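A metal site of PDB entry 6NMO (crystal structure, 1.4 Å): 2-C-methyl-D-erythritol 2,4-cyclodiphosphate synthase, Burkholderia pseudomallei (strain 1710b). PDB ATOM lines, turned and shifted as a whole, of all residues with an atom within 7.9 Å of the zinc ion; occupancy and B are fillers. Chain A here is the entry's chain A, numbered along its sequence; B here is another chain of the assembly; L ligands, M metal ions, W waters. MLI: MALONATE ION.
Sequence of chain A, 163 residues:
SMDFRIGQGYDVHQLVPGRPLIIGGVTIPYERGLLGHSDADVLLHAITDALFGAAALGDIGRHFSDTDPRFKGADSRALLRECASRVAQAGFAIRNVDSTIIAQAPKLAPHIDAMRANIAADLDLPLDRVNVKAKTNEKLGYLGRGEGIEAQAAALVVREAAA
The side-chain carboxylate (OD1) of Asp 11 lies within salt-bridge range of the side-chain amino group (NZ) of Lys 135 of chain B (3.6 Å). The backbone carbonyl oxygen of Leu 35 lies within hydrogen-bond range of a ring nitrogen (ND1) of His 13, 2.8 Å away. A ring nitrogen (NE2) of His 45 lies close to the side-chain hydroxyl (OG) of Ser 38 (3.3 Å). A ring nitrogen (NE2) of His 45 lies within hydrogen-bond range of the side-chain hydroxyl of Ser 76 (2.9 Å).
Of the 22 residues printed, 3 come within 4 Å of the zinc ion. The nearest printed residue that does not touch the zinc ion is Val 12 (4.9 Å).
The zinc ion is bound by OD2 of Asp 11 (2.0 Å), NE2 of His 13 (2.1 Å), ND1 of His 45 (2.1 Å), O7 of the ligand (2.2 Å), water W2 (2.2 Å) and water W1 (2.4 Å).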
ATOM      1  N   TYR A  10       4.276  19.615  -1.988  1.00  0.00           N
ATOM      2  CA  TYR A  10       4.183  21.064  -2.023  1.00  0.00           C
ATOM      3  C   TYR A  10       2.915  21.473  -1.298  1.00  0.00           C
ATOM      4  O   TYR A  10       1.877  20.825  -1.462  1.00  0.00           O
ATOM      5  CB  TYR A  10       4.043  21.515  -3.486  1.00  0.00           C
ATOM      6  CG  TYR A  10       3.584  22.947  -3.684  1.00  0.00           C
ATOM      7  CD1 TYR A  10       4.475  24.002  -3.597  1.00  0.00           C
ATOM      8  CD2 TYR A  10       2.239  23.258  -3.913  1.00  0.00           C
ATOM      9  CE1 TYR A  10       4.068  25.301  -3.769  1.00  0.00           C
ATOM     10  CE2 TYR A  10       1.825  24.564  -4.071  1.00  0.00           C
ATOM     11  CZ  TYR A  10       2.751  25.584  -3.998  1.00  0.00           C
ATOM     12  OH  TYR A  10       2.386  26.912  -4.160  1.00  0.00           O
ATOM     13  N   ASP A  11       2.982  22.575  -0.560  1.00  0.00           N
ATOM     14  CA  ASP A  11       1.749  23.162  -0.055  1.00  0.00           C
ATOM     15  C   ASP A  11       1.930  24.664   0.148  1.00  0.00           C
ATOM     16  O   ASP A  11       3.056  25.158   0.289  1.00  0.00           O
ATOM     17  CB  ASP A  11       1.320  22.486   1.239  1.00  0.00           C
ATOM     18  CG  ASP A  11      -0.144  22.707   1.548  1.00  0.00           C
ATOM     19  OD1 ASP A  11      -0.931  22.985   0.608  1.00  0.00           O
ATOM     20  OD2 ASP A  11      -0.507  22.627   2.736  1.00  0.00           O
ATOM     21  N   VAL A  12       0.812  25.380   0.159  1.00  0.00           N
ATOM     22  CA  VAL A  12       0.793  26.793   0.480  1.00  0.00           C
ATOM     23  C   VAL A  12      -0.515  27.103   1.186  1.00  0.00           C
ATOM     24  O   VAL A  12      -1.567  26.541   0.854  1.00  0.00           O
ATOM     25  CB  VAL A  12       0.980  27.665  -0.788  1.00  0.00           C
ATOM     26  CG1 VAL A  12      -0.207  27.533  -1.734  1.00  0.00           C
ATOM     27  CG2 VAL A  12       1.244  29.124  -0.407  1.00  0.00           C
ATOM     28  N   HIS A  13      -0.459  28.023   2.159  1.00  0.00           N
ATOM     29  CA  HIS A  13      -1.664  28.525   2.797  1.00  0.00           C
ATOM     30  C   HIS A  13      -1.540  30.026   2.969  1.00  0.00           C
ATOM     31  O   HIS A  13      -0.441  30.551   3.174  1.00  0.00           O
ATOM     32  CB  HIS A  13      -1.883  27.893   4.185  1.00  0.00           C
ATOM     33  CG  HIS A  13      -2.375  26.488   4.130  1.00  0.00           C
ATOM     34  ND1 HIS A  13      -3.706  26.157   4.255  1.00  0.00           N
ATOM     35  CD2 HIS A  13      -1.718  25.314   3.939  1.00  0.00           C
ATOM     36  CE1 HIS A  13      -3.851  24.850   4.159  1.00  0.00           C
ATOM     37  NE2 HIS A  13      -2.658  24.310   3.972  1.00  0.00           N
ATOM     38  N   LEU A  35      -4.500  29.937   7.143  1.00  0.00           N
ATOM     39  CA  LEU A  35      -5.916  29.704   6.894  1.00  0.00           C
ATOM     40  C   LEU A  35      -6.096  28.372   6.201  1.00  0.00           C
ATOM     41  O   LEU A  35      -5.486  28.103   5.153  1.00  0.00           O
ATOM     42  CB  LEU A  35      -6.450  30.812   5.983  1.00  0.00           C
ATOM     43  CG  LEU A  35      -7.882  30.618   5.515  1.00  0.00           C
ATOM     44  CD1 LEU A  35      -8.821  30.665   6.700  1.00  0.00           C
ATOM     45  CD2 LEU A  35      -8.272  31.673   4.480  1.00  0.00           C
ATOM     46  N   GLY A  36      -6.940  27.525   6.774  1.00  0.00           N
ATOM     47  CA  GLY A  36      -7.251  26.246   6.170  1.00  0.00           C
ATOM     48  C   GLY A  36      -8.407  25.596   6.894  1.00  0.00           C
ATOM     49  O   GLY A  36      -8.853  26.060   7.940  1.00  0.00           O
ATOM     50  N   HIS A  37      -8.868  24.492   6.311  1.00  0.00           N
ATOM     51  CA  HIS A  37      -9.925  23.700   6.942  1.00  0.00           C
ATOM     52  C   HIS A  37      -9.390  23.024   8.207  1.00  0.00           C
ATOM     53  O   HIS A  37     -10.070  23.034   9.252  1.00  0.00           O
ATOM     54  CB  HIS A  37     -10.410  22.669   5.922  1.00  0.00           C
ATOM     55  CG  HIS A  37     -11.521  21.793   6.399  1.00  0.00           C
ATOM     56  ND1 HIS A  37     -12.783  22.277   6.653  1.00  0.00           N
ATOM     57  CD2 HIS A  37     -11.563  20.463   6.617  1.00  0.00           C
ATOM     58  CE1 HIS A  37     -13.560  21.270   7.017  1.00  0.00           C
ATOM     59  NE2 HIS A  37     -12.852  20.163   7.008  1.00  0.00           N
ATOM     60  N   SER A  38      -8.189  22.449   8.132  1.00  0.00           N
ATOM     61  CA  SER A  38      -7.505  21.852   9.278  1.00  0.00           C
ATOM     62  C   SER A  38      -6.781  22.954  10.047  1.00  0.00           C
ATOM     63  O   SER A  38      -7.072  24.144   9.833  1.00  0.00           O
ATOM     64  CB  SER A  38      -6.485  20.819   8.793  1.00  0.00           C
ATOM     65  OG  SER A  38      -5.407  21.417   8.072  1.00  0.00           O
ATOM     66  N   ASP A  39      -5.840  22.591  10.904  1.00  0.00           N
ATOM     67  CA  ASP A  39      -4.990  23.621  11.505  1.00  0.00           C
ATOM     68  C   ASP A  39      -4.062  24.307  10.484  1.00  0.00           C
ATOM     69  O   ASP A  39      -3.362  25.240  10.865  1.00  0.00           O
ATOM     70  CB  ASP A  39      -4.193  23.069  12.699  1.00  0.00           C
ATOM     71  CG  ASP A  39      -3.147  22.033  12.307  1.00  0.00           C
ATOM     72  OD1 ASP A  39      -2.851  21.844  11.108  1.00  0.00           O
ATOM     73  OD2 ASP A  39      -2.594  21.402  13.234  1.00  0.00           O
ATOM     74  N   ALA A  40      -4.048  23.843   9.224  1.00  0.00           N
ATOM     75  CA  ALA A  40      -3.390  24.540   8.123  1.00  0.00           C
ATOM     76  C   ALA A  40      -1.869  24.465   8.182  1.00  0.00           C
ATOM     77  O   ALA A  40      -1.169  25.350   7.662  1.00  0.00           O
ATOM     78  CB  ALA A  40      -3.894  25.983   7.960  1.00  0.00           C
ATOM     79  N   ASP A  41      -1.333  23.414   8.812  1.00  0.00           N
ATOM     80  CA  ASP A  41       0.107  23.271   8.994  1.00  0.00           C
ATOM     81  C   ASP A  41       0.745  22.945   7.654  1.00  0.00           C
ATOM     82  O   ASP A  41       0.861  21.789   7.268  1.00  0.00           O
ATOM     83  CB  ASP A  41       0.402  22.219  10.061  1.00  0.00           C
ATOM     84  CG  ASP A  41       1.840  22.190  10.494  1.00  0.00           C
ATOM     85  OD1 ASP A  41       2.738  22.419   9.642  1.00  0.00           O
ATOM     86  OD2 ASP A  41       2.067  21.899  11.689  1.00  0.00           O
ATOM     87  N   VAL A  42       1.194  23.988   6.960  1.00  0.00           N
ATOM     88  CA  VAL A  42       1.658  23.855   5.578  1.00  0.00           C
ATOM     89  C   VAL A  42       2.841  22.904   5.463  1.00  0.00           C
ATOM     90  O   VAL A  42       2.962  22.150   4.473  1.00  0.00           O
ATOM     91  CB  VAL A  42       1.959  25.261   5.010  1.00  0.00           C
ATOM     92  CG1 VAL A  42       3.131  25.920   5.718  1.00  0.00           C
ATOM     93  CG2 VAL A  42       2.210  25.225   3.510  1.00  0.00           C
ATOM     94  N   LEU A  43       3.734  22.906   6.450  1.00  0.00           N
ATOM     95  CA  LEU A  43       4.901  22.026   6.394  1.00  0.00           C
ATOM     96  C   LEU A  43       4.486  20.572   6.538  1.00  0.00           C
ATOM     97  O   LEU A  43       4.924  19.700   5.761  1.00  0.00           O
ATOM     98  CB  LEU A  43       5.909  22.404   7.482  1.00  0.00           C
ATOM     99  CG  LEU A  43       7.130  21.480   7.596  1.00  0.00           C
ATOM    100  CD1 LEU A  43       7.947  21.451   6.300  1.00  0.00           C
ATOM    101  CD2 LEU A  43       8.030  21.919   8.753  1.00  0.00           C
ATOM    102  N   LEU A  44       3.660  20.262   7.546  1.00  0.00           N
ATOM    103  CA  LEU A  44       3.227  18.875   7.684  1.00  0.00           C
ATOM    104  C   LEU A  44       2.418  18.399   6.479  1.00  0.00           C
ATOM    105  O   LEU A  44       2.531  17.226   6.092  1.00  0.00           O
ATOM    106  CB  LEU A  44       2.461  18.684   8.996  1.00  0.00           C
ATOM    107  CG  LEU A  44       3.289  19.008  10.247  1.00  0.00           C
ATOM    108  CD1 LEU A  44       2.524  18.575  11.473  1.00  0.00           C
ATOM    109  CD2 LEU A  44       4.662  18.324  10.189  1.00  0.00           C
ATOM    110  N   HIS A  45       1.624  19.286   5.863  1.00  0.00           N
ATOM    111  CA  HIS A  45       0.881  18.864   4.676  1.00  0.00           C
ATOM    112  C   HIS A  45       1.815  18.512   3.531  1.00  0.00           C
ATOM    113  O   HIS A  45       1.572  17.531   2.811  1.00  0.00           O
ATOM    114  CB  HIS A  45      -0.082  19.965   4.217  1.00  0.00           C
ATOM    115  CG  HIS A  45      -1.173  20.242   5.199  1.00  0.00           C
ATOM    116  ND1 HIS A  45      -2.099  21.239   5.013  1.00  0.00           N
ATOM    117  CD2 HIS A  45      -1.463  19.664   6.395  1.00  0.00           C
ATOM    118  CE1 HIS A  45      -2.931  21.251   6.046  1.00  0.00           C
ATOM    119  NE2 HIS A  45      -2.556  20.323   6.900  1.00  0.00           N
ATOM    120  N   ALA A  46       2.864  19.312   3.332  1.00  0.00           N
ATOM    121  CA  ALA A  46       3.811  19.003   2.259  1.00  0.00           C
ATOM    122  C   ALA A  46       4.486  17.663   2.502  1.00  0.00           C
ATOM    123  O   ALA A  46       4.655  16.858   1.569  1.00  0.00           O
ATOM    124  CB  ALA A  46       4.842  20.114   2.111  1.00  0.00           C
ATOM    125  N   ASP A  49       2.067  14.828   1.801  1.00  0.00           N
ATOM    126  CA  ASP A  49       1.919  14.584   0.365  1.00  0.00           C
ATOM    127  C   ASP A  49       3.119  13.834  -0.189  1.00  0.00           C
ATOM    128  O   ASP A  49       2.962  12.925  -1.023  1.00  0.00           O
ATOM    129  CB  ASP A  49       1.708  15.909  -0.379  1.00  0.00           C
ATOM    130  CG  ASP A  49       0.337  16.034  -0.997  1.00  0.00           C
ATOM    131  OD1 ASP A  49      -0.523  15.184  -0.737  1.00  0.00           O
ATOM    132  OD2 ASP A  49       0.126  17.002  -1.753  1.00  0.00           O
ATOM    133  N   ILE A  60      -2.930  14.085  -0.051  1.00  0.00           N
ATOM    134  CA  ILE A  60      -3.546  14.433   1.234  1.00  0.00           C
ATOM    135  C   ILE A  60      -5.035  14.712   1.062  1.00  0.00           C
ATOM    136  O   ILE A  60      -5.842  14.363   1.935  1.00  0.00           O
ATOM    137  CB  ILE A  60      -2.774  15.584   1.900  1.00  0.00           C
ATOM    138  CG1 ILE A  60      -3.220  15.764   3.348  1.00  0.00           C
ATOM    139  CG2 ILE A  60      -2.891  16.890   1.095  1.00  0.00           C
ATOM    140  CD1 ILE A  60      -2.409  16.841   4.119  1.00  0.00           C
ATOM    141  N   ASP A  66     -10.745  18.134   2.552  1.00  0.00           N
ATOM    142  CA  ASP A  66     -10.957  19.450   3.138  1.00  0.00           C
ATOM    143  C   ASP A  66     -12.415  19.876   3.135  1.00  0.00           C
ATOM    144  O   ASP A  66     -12.730  20.986   3.569  1.00  0.00           O
ATOM    145  CB  ASP A  66     -10.059  20.508   2.461  1.00  0.00           C
ATOM    146  CG  ASP A  66     -10.534  20.917   1.076  1.00  0.00           C
ATOM    147  OD1 ASP A  66     -10.017  21.930   0.561  1.00  0.00           O
ATOM    148  OD2 ASP A  66     -11.422  20.249   0.506  1.00  0.00           O
ATOM    149  N   SER A  76      -2.656  18.530  12.376  1.00  0.00           N
ATOM    150  CA  SER A  76      -1.979  17.944  11.234  1.00  0.00           C
ATOM    151  C   SER A  76      -0.903  16.945  11.638  1.00  0.00           C
ATOM    152  O   SER A  76      -0.470  16.152  10.800  1.00  0.00           O
ATOM    153  CB  SER A  76      -1.412  19.035  10.327  1.00  0.00           C
ATOM    154  OG  SER A  76      -2.479  19.743   9.716  1.00  0.00           O
ATOM    155  N   LYS B 135      -3.706  19.782  -6.410  1.00  0.00           N
ATOM    156  CA  LYS B 135      -4.236  20.719  -5.416  1.00  0.00           C
ATOM    157  C   LYS B 135      -4.359  22.107  -6.027  1.00  0.00           C
ATOM    158  O   LYS B 135      -3.852  22.377  -7.119  1.00  0.00           O
ATOM    159  CB  LYS B 135      -3.314  20.796  -4.212  1.00  0.00           C
ATOM    160  CG  LYS B 135      -1.899  21.282  -4.627  1.00  0.00           C
ATOM    161  CD  LYS B 135      -0.954  21.281  -3.468  1.00  0.00           C
ATOM    162  CE  LYS B 135      -0.950  19.916  -2.810  1.00  0.00           C
ATOM    163  NZ  LYS B 135      -0.676  19.917  -1.335  1.00  0.00           N
ATOM    164  N   GLU B 138      -4.602  27.908  -3.225  1.00  0.00           N
ATOM    165  CA  GLU B 138      -5.231  28.700  -2.167  1.00  0.00           C
ATOM    166  C   GLU B 138      -5.415  30.155  -2.581  1.00  0.00           C
ATOM    167  O   GLU B 138      -5.290  31.088  -1.782  1.00  0.00           O
ATOM    168  CB  GLU B 138      -4.458  28.568  -0.841  1.00  0.00           C
ATOM    169  CG  GLU B 138      -4.558  27.181  -0.238  1.00  0.00           C
ATOM    170  CD  GLU B 138      -5.950  26.904   0.256  1.00  0.00           C
ATOM    171  OE1 GLU B 138      -6.512  27.763   0.971  1.00  0.00           O
ATOM    172  OE2 GLU B 138      -6.505  25.834  -0.060  1.00  0.00           O
HETATM  173  C1  MLI L   1      -6.658  21.078   4.179  1.00  0.00           C
HETATM  174  C2  MLI L   1      -5.217  20.990   3.676  1.00  0.00           C
HETATM  175  C3  MLI L   1      -6.875  22.447   4.788  1.00  0.00           C
HETATM  176  O6  MLI L   1      -4.737  19.863   3.459  1.00  0.00           O
HETATM  177  O7  MLI L   1      -4.600  22.063   3.491  1.00  0.00           O
HETATM  178  O8  MLI L   1      -7.593  23.269   4.180  1.00  0.00           O
HETATM  179  O9  MLI L   1      -6.301  22.696   5.858  1.00  0.00           O
HETATM  180 ZN    ZN M   1      -2.458  22.380   3.267  1.00  0.00          ZN
HETATM  181  O   HOH W   1      -3.215  23.326   1.210  1.00  0.00           O
HETATM  182  O   HOH W   2      -2.608  20.518   2.063  1.00  0.00           O
